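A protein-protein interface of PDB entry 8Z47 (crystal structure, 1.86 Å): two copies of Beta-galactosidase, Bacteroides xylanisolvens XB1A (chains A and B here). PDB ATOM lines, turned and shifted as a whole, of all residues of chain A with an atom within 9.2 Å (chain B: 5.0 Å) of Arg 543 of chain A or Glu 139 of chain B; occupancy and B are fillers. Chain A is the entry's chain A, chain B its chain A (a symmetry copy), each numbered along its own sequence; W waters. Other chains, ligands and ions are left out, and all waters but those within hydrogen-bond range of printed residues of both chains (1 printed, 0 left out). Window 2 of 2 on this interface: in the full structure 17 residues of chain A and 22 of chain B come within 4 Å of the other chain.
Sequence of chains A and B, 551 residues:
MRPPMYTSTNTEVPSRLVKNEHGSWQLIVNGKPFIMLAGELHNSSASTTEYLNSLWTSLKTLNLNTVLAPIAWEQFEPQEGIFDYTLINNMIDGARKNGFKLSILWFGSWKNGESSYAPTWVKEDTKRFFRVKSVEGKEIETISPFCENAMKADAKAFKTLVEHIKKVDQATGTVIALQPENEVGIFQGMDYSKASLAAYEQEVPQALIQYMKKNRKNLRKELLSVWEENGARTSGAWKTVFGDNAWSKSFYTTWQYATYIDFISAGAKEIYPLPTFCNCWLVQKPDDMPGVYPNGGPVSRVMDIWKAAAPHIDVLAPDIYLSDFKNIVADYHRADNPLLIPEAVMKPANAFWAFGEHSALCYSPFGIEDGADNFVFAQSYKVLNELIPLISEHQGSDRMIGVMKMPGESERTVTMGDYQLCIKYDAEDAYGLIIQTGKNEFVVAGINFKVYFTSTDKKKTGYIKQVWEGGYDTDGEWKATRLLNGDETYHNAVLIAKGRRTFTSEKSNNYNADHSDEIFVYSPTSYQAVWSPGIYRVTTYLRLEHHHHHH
The guanidinium group (NH1) of Arg 131 of chain B lies close to the guanidinium group (NH2) of Arg 543 of chain A (3.3 Å).
The side-chain hydroxyl of Tyr 541 of chain A lies within hydrogen-bond range of the guanidinium group of Arg 131 of chain B.
The guanidinium group of Arg 543 of chain A is in salt-bridge range of the side-chain carboxylate of Glu 141 of chain B (2.7 Å).
The guanidinium group (NH1) of Arg 543 of chain A sits at hydrogen-bond distance from the backbone carbonyl oxygen (O) of Glu 139 of chain B, 3.2 Å away.
The side-chain hydroxyl (OH) of Tyr 541 of chain A sits at hydrogen-bond distance from the side-chain carboxylate (OE2) of Glu 141 of chain B (2.4 Å).
N of Tyr 541 of chain A sits at hydrogen-bond distance from O of Tyr 463 of chain A, 3.0 Å away.
The backbone carbonyl oxygen (O) of Val 132 of chain B sits at hydrogen-bond distance from the backbone NH (N) of Ile 140 of chain B.
The side-chain hydroxyl (OH) of Tyr 419 of chain A sits at hydrogen-bond distance from the backbone NH (N) of Tyr 541 of chain A (3.2 Å).
NH1 of Arg 131 of chain B lies within hydrogen-bond range of O of Ile 140 of chain B (3.1 Å).
The backbone carbonyl oxygen of Thr 461 of chain A sits at hydrogen-bond distance from the backbone NH of Arg 543 of chain A.
OE1 of Glu 141 of chain B is in salt-bridge range of NH1 of Arg 131 of chain B (3.0 Å).
Among the printed residues, pairs that only touch across the chains: Tyr 463 of chain A with Glu 141 of chain B (3.6 Å), Arg 543 of chain A with Thr 126 of chain B (3.7 Å) and Arg 543 of chain A with Ile 140 of chain B (3.9 Å).
Printed residues of chain B within 4 Å of Tyr 463 of chain A: Glu 141 (3.6 Å).
Of the printed residues of chain B, Tyr 541 of chain A touches Arg 131 (3.0 Å) and Glu 141 (2.4 Å).
Of the printed residues of chain A, Arg 131 of chain B touches Tyr 541 and Arg 543.
Of chain A, only Arg 543 comes within 4 Å of Glu 139 of chain B.
Of the printed residues of chain A, Ile 140 of chain B touches Arg 543 (3.9 Å).
Of the printed residues of chain A, Glu 141 of chain B touches Tyr 463, Tyr 541 and Arg 543.
The nearest printed residue of chain B that does not touch Arg 543 of chain A is Lys 138 of chain B (6.2 Å).
The nearest printed residue of chain A that does not touch Arg 131 of chain B is Tyr 463 of chain A (6.8 Å).
Of the 16 printed residues of chain A, 3 touch a printed residue of chain B.
Hydrophobic or aromatic side chains of chain A within 4 Å of the printed part of chain B: Tyr 463 and Tyr 541.
Along chain A the printed residues that touch a printed residue of chain B span positions 463 to 543.
Among the printed residues, 8 pairs touch across the chains.
Among the printed residues, Asp or Glu carboxylates within 4 Å of a Lys or Arg side-chain nitrogen of the other chain: Arg 543 of chain A with Glu 141 of chain B.
No position is printed for both chains.
Of the 8 pairs that touch across the chains among the printed residues, none has its exchanged pair printed and touching as well.
Water W1 lies within hydrogen-bond range of O of Ile 464 of chain A (2.7 Å), OE2 of Glu 141 of chain B (3.0 Å) and ND2 of Asn 492 of chain A (3.0 Å).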
ATOM      1  N   TYR A 419      -5.675  23.846  -9.869  1.00  0.00           N
ATOM      2  CA  TYR A 419      -5.968  24.863 -10.857  1.00  0.00           C
ATOM      3  C   TYR A 419      -6.743  26.020 -10.262  1.00  0.00           C
ATOM      4  O   TYR A 419      -7.496  25.865  -9.299  1.00  0.00           O
ATOM      5  CB  TYR A 419      -6.727  24.226 -12.015  1.00  0.00           C
ATOM      6  CG  TYR A 419      -5.907  23.173 -12.746  1.00  0.00           C
ATOM      7  CD1 TYR A 419      -5.042  23.504 -13.777  1.00  0.00           C
ATOM      8  CD2 TYR A 419      -6.032  21.834 -12.424  1.00  0.00           C
ATOM      9  CE1 TYR A 419      -4.251  22.546 -14.391  1.00  0.00           C
ATOM     10  CE2 TYR A 419      -5.293  20.861 -13.066  1.00  0.00           C
ATOM     11  CZ  TYR A 419      -4.407  21.215 -14.072  1.00  0.00           C
ATOM     12  OH  TYR A 419      -3.745  20.198 -14.688  1.00  0.00           O
ATOM     13  N   ASN A 440      -7.199  16.244 -13.063  1.00  0.00           N
ATOM     14  CA  ASN A 440      -6.961  17.016 -14.286  1.00  0.00           C
ATOM     15  C   ASN A 440      -8.160  16.939 -15.239  1.00  0.00           C
ATOM     16  O   ASN A 440      -8.014  16.926 -16.478  1.00  0.00           O
ATOM     17  CB  ASN A 440      -5.697  16.609 -15.021  1.00  0.00           C
ATOM     18  CG  ASN A 440      -4.477  16.760 -14.145  1.00  0.00           C
ATOM     19  OD1 ASN A 440      -4.009  17.874 -13.893  1.00  0.00           O
ATOM     20  ND2 ASN A 440      -3.998  15.649 -13.626  1.00  0.00           N
ATOM     21  N   SER A 455      -2.397  27.378 -13.316  1.00  0.00           N
ATOM     22  CA  SER A 455      -1.797  26.613 -12.245  1.00  0.00           C
ATOM     23  C   SER A 455      -1.900  27.364 -10.922  1.00  0.00           C
ATOM     24  O   SER A 455      -1.514  28.527 -10.860  1.00  0.00           O
ATOM     25  CB  SER A 455      -0.341  26.363 -12.560  1.00  0.00           C
ATOM     26  OG  SER A 455       0.207  25.452 -11.621  1.00  0.00           O
ATOM     27  N   ASP A 457      -0.098  26.538  -8.300  1.00  0.00           N
ATOM     28  CA  ASP A 457       1.355  26.677  -7.999  1.00  0.00           C
ATOM     29  C   ASP A 457       2.020  27.496  -9.104  1.00  0.00           C
ATOM     30  O   ASP A 457       2.036  27.041 -10.253  1.00  0.00           O
ATOM     31  CB  ASP A 457       1.973  25.301  -7.830  1.00  0.00           C
ATOM     32  CG  ASP A 457       3.483  25.238  -7.645  1.00  0.00           C
ATOM     33  OD1 ASP A 457       4.123  26.305  -7.590  1.00  0.00           O
ATOM     34  OD2 ASP A 457       4.002  24.112  -7.550  1.00  0.00           O
ATOM     35  N   LYS A 458       2.622  28.621  -8.736  1.00  0.00           N
ATOM     36  CA  LYS A 458       3.194  29.540  -9.749  1.00  0.00           C
ATOM     37  C   LYS A 458       4.553  29.034 -10.254  1.00  0.00           C
ATOM     38  O   LYS A 458       5.119  29.690 -11.143  1.00  0.00           O
ATOM     39  CB  LYS A 458       3.259  30.946  -9.148  1.00  0.00           C
ATOM     40  CG  LYS A 458       1.939  31.417  -8.552  1.00  0.00           C
ATOM     41  CD  LYS A 458       0.754  31.338  -9.509  1.00  0.00           C
ATOM     42  CE  LYS A 458      -0.502  31.888  -8.909  1.00  0.00           C
ATOM     43  NZ  LYS A 458      -1.607  30.927  -8.941  1.00  0.00           N
ATOM     44  N   LYS A 459       5.038  27.908  -9.743  1.00  0.00           N
ATOM     45  CA  LYS A 459       6.288  27.349 -10.310  1.00  0.00           C
ATOM     46  C   LYS A 459       5.898  26.522 -11.530  1.00  0.00           C
ATOM     47  O   LYS A 459       6.791  26.112 -12.287  1.00  0.00           O
ATOM     48  CB  LYS A 459       6.991  26.433  -9.305  1.00  0.00           C
ATOM     49  CG  LYS A 459       7.819  27.154  -8.258  1.00  0.00           C
ATOM     50  CD  LYS A 459       7.411  26.822  -6.829  1.00  0.00           C
ATOM     51  CE  LYS A 459       8.370  27.400  -5.839  1.00  0.00           C
ATOM     52  NZ  LYS A 459       9.685  27.651  -6.435  1.00  0.00           N
ATOM     53  N   LYS A 460       4.596  26.302 -11.700  1.00  0.00           N
ATOM     54  CA  LYS A 460       4.140  25.427 -12.799  1.00  0.00           C
ATOM     55  C   LYS A 460       3.262  26.184 -13.790  1.00  0.00           C
ATOM     56  O   LYS A 460       2.681  27.209 -13.403  1.00  0.00           O
ATOM     57  CB  LYS A 460       3.333  24.262 -12.226  1.00  0.00           C
ATOM     58  CG  LYS A 460       4.150  23.171 -11.563  1.00  0.00           C
ATOM     59  CD  LYS A 460       3.349  22.411 -10.514  1.00  0.00           C
ATOM     60  CE  LYS A 460       3.614  20.945 -10.563  1.00  0.00           C
ATOM     61  NZ  LYS A 460       3.125  20.273  -9.357  1.00  0.00           N
ATOM     62  N   THR A 461       3.240  25.716 -15.031  1.00  0.00           N
ATOM     63  CA  THR A 461       2.344  26.248 -16.052  1.00  0.00           C
ATOM     64  C   THR A 461       1.195  25.263 -16.304  1.00  0.00           C
ATOM     65  O   THR A 461       1.410  24.113 -16.703  1.00  0.00           O
ATOM     66  CB  THR A 461       3.124  26.533 -17.341  1.00  0.00           C
ATOM     67  OG1 THR A 461       3.866  27.728 -17.118  1.00  0.00           O
ATOM     68  CG2 THR A 461       2.220  26.805 -18.532  1.00  0.00           C
ATOM     69  N   GLY A 462      -0.040  25.730 -16.077  1.00  0.00           N
ATOM     70  CA  GLY A 462      -1.224  24.920 -16.338  1.00  0.00           C
ATOM     71  C   GLY A 462      -1.933  25.355 -17.629  1.00  0.00           C
ATOM     72  O   GLY A 462      -1.996  26.539 -17.948  1.00  0.00           O
ATOM     73  N   TYR A 463      -2.484  24.379 -18.354  1.00  0.00           N
ATOM     74  CA  TYR A 463      -3.151  24.634 -19.621  1.00  0.00           C
ATOM     75  C   TYR A 463      -4.266  23.626 -19.866  1.00  0.00           C
ATOM     76  O   TYR A 463      -4.226  22.522 -19.333  1.00  0.00           O
ATOM     77  CB  TYR A 463      -2.093  24.447 -20.717  1.00  0.00           C
ATOM     78  CG  TYR A 463      -2.169  25.556 -21.750  1.00  0.00           C
ATOM     79  CD1 TYR A 463      -1.726  26.835 -21.429  1.00  0.00           C
ATOM     80  CD2 TYR A 463      -2.749  25.356 -22.995  1.00  0.00           C
ATOM     81  CE1 TYR A 463      -1.843  27.884 -22.322  1.00  0.00           C
ATOM     82  CE2 TYR A 463      -2.836  26.389 -23.912  1.00  0.00           C
ATOM     83  CZ  TYR A 463      -2.373  27.654 -23.580  1.00  0.00           C
ATOM     84  OH  TYR A 463      -2.465  28.715 -24.454  1.00  0.00           O
ATOM     85  N   ILE A 464      -5.234  23.986 -20.721  1.00  0.00           N
ATOM     86  CA  ILE A 464      -6.170  23.019 -21.268  1.00  0.00           C
ATOM     87  C   ILE A 464      -5.385  22.011 -22.101  1.00  0.00           C
ATOM     88  O   ILE A 464      -4.557  22.407 -22.927  1.00  0.00           O
ATOM     89  CB  ILE A 464      -7.245  23.710 -22.131  1.00  0.00           C
ATOM     90  CG1 ILE A 464      -8.234  24.501 -21.265  1.00  0.00           C
ATOM     91  CG2 ILE A 464      -7.946  22.693 -23.042  1.00  0.00           C
ATOM     92  CD1 ILE A 464      -9.096  25.495 -22.019  1.00  0.00           C
ATOM     93  N   ASN A 492      -6.907  26.176 -27.424  1.00  0.00           N
ATOM     94  CA  ASN A 492      -6.843  25.695 -26.058  1.00  0.00           C
ATOM     95  C   ASN A 492      -6.418  26.784 -25.084  1.00  0.00           C
ATOM     96  O   ASN A 492      -6.009  26.463 -23.971  1.00  0.00           O
ATOM     97  CB  ASN A 492      -6.081  24.388 -25.937  1.00  0.00           C
ATOM     98  CG  ASN A 492      -6.765  23.218 -26.605  1.00  0.00           C
ATOM     99  OD1 ASN A 492      -7.952  23.264 -26.972  1.00  0.00           O
ATOM    100  ND2 ASN A 492      -6.012  22.150 -26.801  1.00  0.00           N
ATOM    101  N   THR A 540      -7.040  18.942 -18.425  1.00  0.00           N
ATOM    102  CA  THR A 540      -5.999  19.949 -18.266  1.00  0.00           C
ATOM    103  C   THR A 540      -4.703  19.234 -17.963  1.00  0.00           C
ATOM    104  O   THR A 540      -4.721  18.014 -17.778  1.00  0.00           O
ATOM    105  CB  THR A 540      -6.393  20.855 -17.105  1.00  0.00           C
ATOM    106  OG1 THR A 540      -6.612  20.001 -15.988  1.00  0.00           O
ATOM    107  CG2 THR A 540      -7.649  21.659 -17.388  1.00  0.00           C
ATOM    108  N   TYR A 541      -3.620  19.992 -17.904  1.00  0.00           N
ATOM    109  CA  TYR A 541      -2.299  19.392 -17.605  1.00  0.00           C
ATOM    110  C   TYR A 541      -1.368  20.446 -17.075  1.00  0.00           C
ATOM    111  O   TYR A 541      -1.552  21.640 -17.350  1.00  0.00           O
ATOM    112  CB  TYR A 541      -1.714  18.681 -18.825  1.00  0.00           C
ATOM    113  CG  TYR A 541      -1.091  19.497 -19.950  1.00  0.00           C
ATOM    114  CD1 TYR A 541      -1.865  20.259 -20.812  1.00  0.00           C
ATOM    115  CD2 TYR A 541       0.276  19.442 -20.186  1.00  0.00           C
ATOM    116  CE1 TYR A 541      -1.295  20.970 -21.855  1.00  0.00           C
ATOM    117  CE2 TYR A 541       0.858  20.147 -21.224  1.00  0.00           C
ATOM    118  CZ  TYR A 541       0.071  20.911 -22.063  1.00  0.00           C
ATOM    119  OH  TYR A 541       0.662  21.596 -23.083  1.00  0.00           O
ATOM    120  N   LEU A 542      -0.385  19.991 -16.312  1.00  0.00           N
ATOM    121  CA  LEU A 542       0.632  20.896 -15.741  1.00  0.00           C
ATOM    122  C   LEU A 542       2.007  20.487 -16.280  1.00  0.00           C
ATOM    123  O   LEU A 542       2.264  19.282 -16.350  1.00  0.00           O
ATOM    124  CB  LEU A 542       0.579  20.733 -14.228  1.00  0.00           C
ATOM    125  CG  LEU A 542      -0.696  21.209 -13.529  1.00  0.00           C
ATOM    126  CD1 LEU A 542      -0.827  20.510 -12.191  1.00  0.00           C
ATOM    127  CD2 LEU A 542      -0.653  22.707 -13.337  1.00  0.00           C
ATOM    128  N   ARG A 543       2.824  21.455 -16.684  1.00  0.00           N
ATOM    129  CA  ARG A 543       4.194  21.147 -17.090  1.00  0.00           C
ATOM    130  C   ARG A 543       5.179  22.036 -16.314  1.00  0.00           C
ATOM    131  O   ARG A 543       4.805  23.200 -16.061  1.00  0.00           O
ATOM    132  CB  ARG A 543       4.391  21.312 -18.599  1.00  0.00           C
ATOM    133  CG  ARG A 543       4.111  22.707 -19.137  1.00  0.00           C
ATOM    134  CD  ARG A 543       4.282  22.801 -20.643  1.00  0.00           C
ATOM    135  NE  ARG A 543       3.283  23.699 -21.232  1.00  0.00           N
ATOM    136  CZ  ARG A 543       3.487  24.974 -21.577  1.00  0.00           C
ATOM    137  NH1 ARG A 543       4.608  25.595 -21.246  1.00  0.00           N
ATOM    138  NH2 ARG A 543       2.555  25.637 -22.240  1.00  0.00           N
ATOM    139  N   THR B 126       7.791  17.811 -22.833  1.00  0.00           N
ATOM    140  CA  THR B 126       8.460  19.028 -23.277  1.00  0.00           C
ATOM    141  C   THR B 126       9.980  18.859 -23.308  1.00  0.00           C
ATOM    142  O   THR B 126      10.665  19.729 -23.830  1.00  0.00           O
ATOM    143  CB  THR B 126       8.056  20.242 -22.449  1.00  0.00           C
ATOM    144  OG1 THR B 126       8.520  19.994 -21.128  1.00  0.00           O
ATOM    145  CG2 THR B 126       6.554  20.466 -22.425  1.00  0.00           C
ATOM    146  N   ARG B 131       9.601  23.247 -26.593  1.00  0.00           N
ATOM    147  CA  ARG B 131       8.768  24.362 -26.983  1.00  0.00           C
ATOM    148  C   ARG B 131       9.595  25.577 -27.420  1.00  0.00           C
ATOM    149  O   ARG B 131      10.761  25.780 -27.069  1.00  0.00           O
ATOM    150  CB  ARG B 131       7.916  24.769 -25.779  1.00  0.00           C
ATOM    151  CG  ARG B 131       7.037  23.700 -25.143  1.00  0.00           C
ATOM    152  CD  ARG B 131       6.088  23.007 -26.124  1.00  0.00           C
ATOM    153  NE  ARG B 131       5.164  22.045 -25.516  1.00  0.00           N
ATOM    154  CZ  ARG B 131       4.132  22.331 -24.750  1.00  0.00           C
ATOM    155  NH1 ARG B 131       3.780  23.581 -24.508  1.00  0.00           N
ATOM    156  NH2 ARG B 131       3.420  21.344 -24.238  1.00  0.00           N
ATOM    157  N   VAL B 132       8.920  26.437 -28.171  1.00  0.00           N
ATOM    158  CA  VAL B 132       9.335  27.805 -28.358  1.00  0.00           C
ATOM    159  C   VAL B 132       9.413  28.488 -26.999  1.00  0.00           C
ATOM    160  O   VAL B 132       8.494  28.358 -26.166  1.00  0.00           O
ATOM    161  CB  VAL B 132       8.335  28.527 -29.287  1.00  0.00           C
ATOM    162  CG1 VAL B 132       8.602  30.018 -29.334  1.00  0.00           C
ATOM    163  CG2 VAL B 132       8.322  27.962 -30.705  1.00  0.00           C
ATOM    164  N   LYS B 133      10.476  29.288 -26.831  1.00  0.00           N
ATOM    165  CA  LYS B 133      10.565  30.240 -25.724  1.00  0.00           C
ATOM    166  C   LYS B 133      10.423  31.680 -26.203  1.00  0.00           C
ATOM    167  O   LYS B 133      10.951  32.072 -27.253  1.00  0.00           O
ATOM    168  CB  LYS B 133      11.913  30.166 -24.990  1.00  0.00           C
ATOM    169  CG  LYS B 133      12.206  28.765 -24.498  1.00  0.00           C
ATOM    170  CD  LYS B 133      13.222  28.678 -23.369  1.00  0.00           C
ATOM    171  CE  LYS B 133      13.472  27.253 -22.983  1.00  0.00           C
ATOM    172  NZ  LYS B 133      14.506  27.213 -21.945  1.00  0.00           N
ATOM    173  N   GLY B 137      11.686  34.302 -21.806  1.00  0.00           N
ATOM    174  CA  GLY B 137      12.179  32.978 -21.373  1.00  0.00           C
ATOM    175  C   GLY B 137      11.080  31.976 -21.071  1.00  0.00           C
ATOM    176  O   GLY B 137      11.402  30.876 -20.605  1.00  0.00           O
ATOM    177  N   LYS B 138       9.833  32.324 -21.367  1.00  0.00           N
ATOM    178  CA  LYS B 138       8.688  31.427 -21.088  1.00  0.00           C
ATOM    179  C   LYS B 138       8.453  30.421 -22.222  1.00  0.00           C
ATOM    180  O   LYS B 138       8.458  30.824 -23.393  1.00  0.00           O
ATOM    181  CB  LYS B 138       7.424  32.265 -20.902  1.00  0.00           C
ATOM    182  CG  LYS B 138       6.711  32.067 -19.577  1.00  0.00           C
ATOM    183  CD  LYS B 138       7.333  32.849 -18.427  1.00  0.00           C
ATOM    184  CE  LYS B 138       7.467  34.308 -18.722  1.00  0.00           C
ATOM    185  NZ  LYS B 138       6.642  35.118 -17.824  1.00  0.00           N
ATOM    186  N   GLU B 139       8.243  29.158 -21.865  1.00  0.00           N
ATOM    187  CA  GLU B 139       7.890  28.138 -22.872  1.00  0.00           C
ATOM    188  C   GLU B 139       6.405  28.313 -23.206  1.00  0.00           C
ATOM    189  O   GLU B 139       5.597  28.409 -22.270  1.00  0.00           O
ATOM    190  CB  GLU B 139       8.169  26.760 -22.292  1.00  0.00           C
ATOM    191  CG  GLU B 139       9.646  26.386 -22.308  1.00  0.00           C
ATOM    192  CD  GLU B 139       9.929  25.167 -21.456  1.00  0.00           C
ATOM    193  OE1 GLU B 139       9.162  24.193 -21.557  1.00  0.00           O
ATOM    194  OE2 GLU B 139      10.917  25.193 -20.694  1.00  0.00           O
ATOM    195  N   ILE B 140       6.071  28.356 -24.489  1.00  0.00           N
ATOM    196  CA  ILE B 140       4.689  28.593 -24.883  1.00  0.00           C
ATOM    197  C   ILE B 140       4.082  27.280 -25.400  1.00  0.00           C
ATOM    198  O   ILE B 140       4.783  26.309 -25.536  1.00  0.00           O
ATOM    199  CB  ILE B 140       4.587  29.762 -25.887  1.00  0.00           C
ATOM    200  CG1 ILE B 140       5.288  29.460 -27.210  1.00  0.00           C
ATOM    201  CG2 ILE B 140       5.094  31.072 -25.259  1.00  0.00           C
ATOM    202  CD1 ILE B 140       5.135  30.571 -28.238  1.00  0.00           C
ATOM    203  N   GLU B 141       2.796  27.312 -25.802  1.00  0.00           N
ATOM    204  CA  GLU B 141       2.041  26.167 -26.289  1.00  0.00           C
ATOM    205  C   GLU B 141       2.270  26.012 -27.791  1.00  0.00           C
ATOM    206  O   GLU B 141       1.312  25.881 -28.570  1.00  0.00           O
ATOM    207  CB  GLU B 141       0.543  26.312 -25.965  1.00  0.00           C
ATOM    208  CG  GLU B 141      -0.230  24.983 -25.937  1.00  0.00           C
ATOM    209  CD  GLU B 141       0.031  24.016 -24.774  1.00  0.00           C
ATOM    210  OE1 GLU B 141       0.886  24.371 -23.966  1.00  0.00           O
ATOM    211  OE2 GLU B 141      -0.560  22.910 -24.694  1.00  0.00           O
HETATM  212  O   HOH W   1      -3.347  22.151 -25.351  1.00  0.00           O
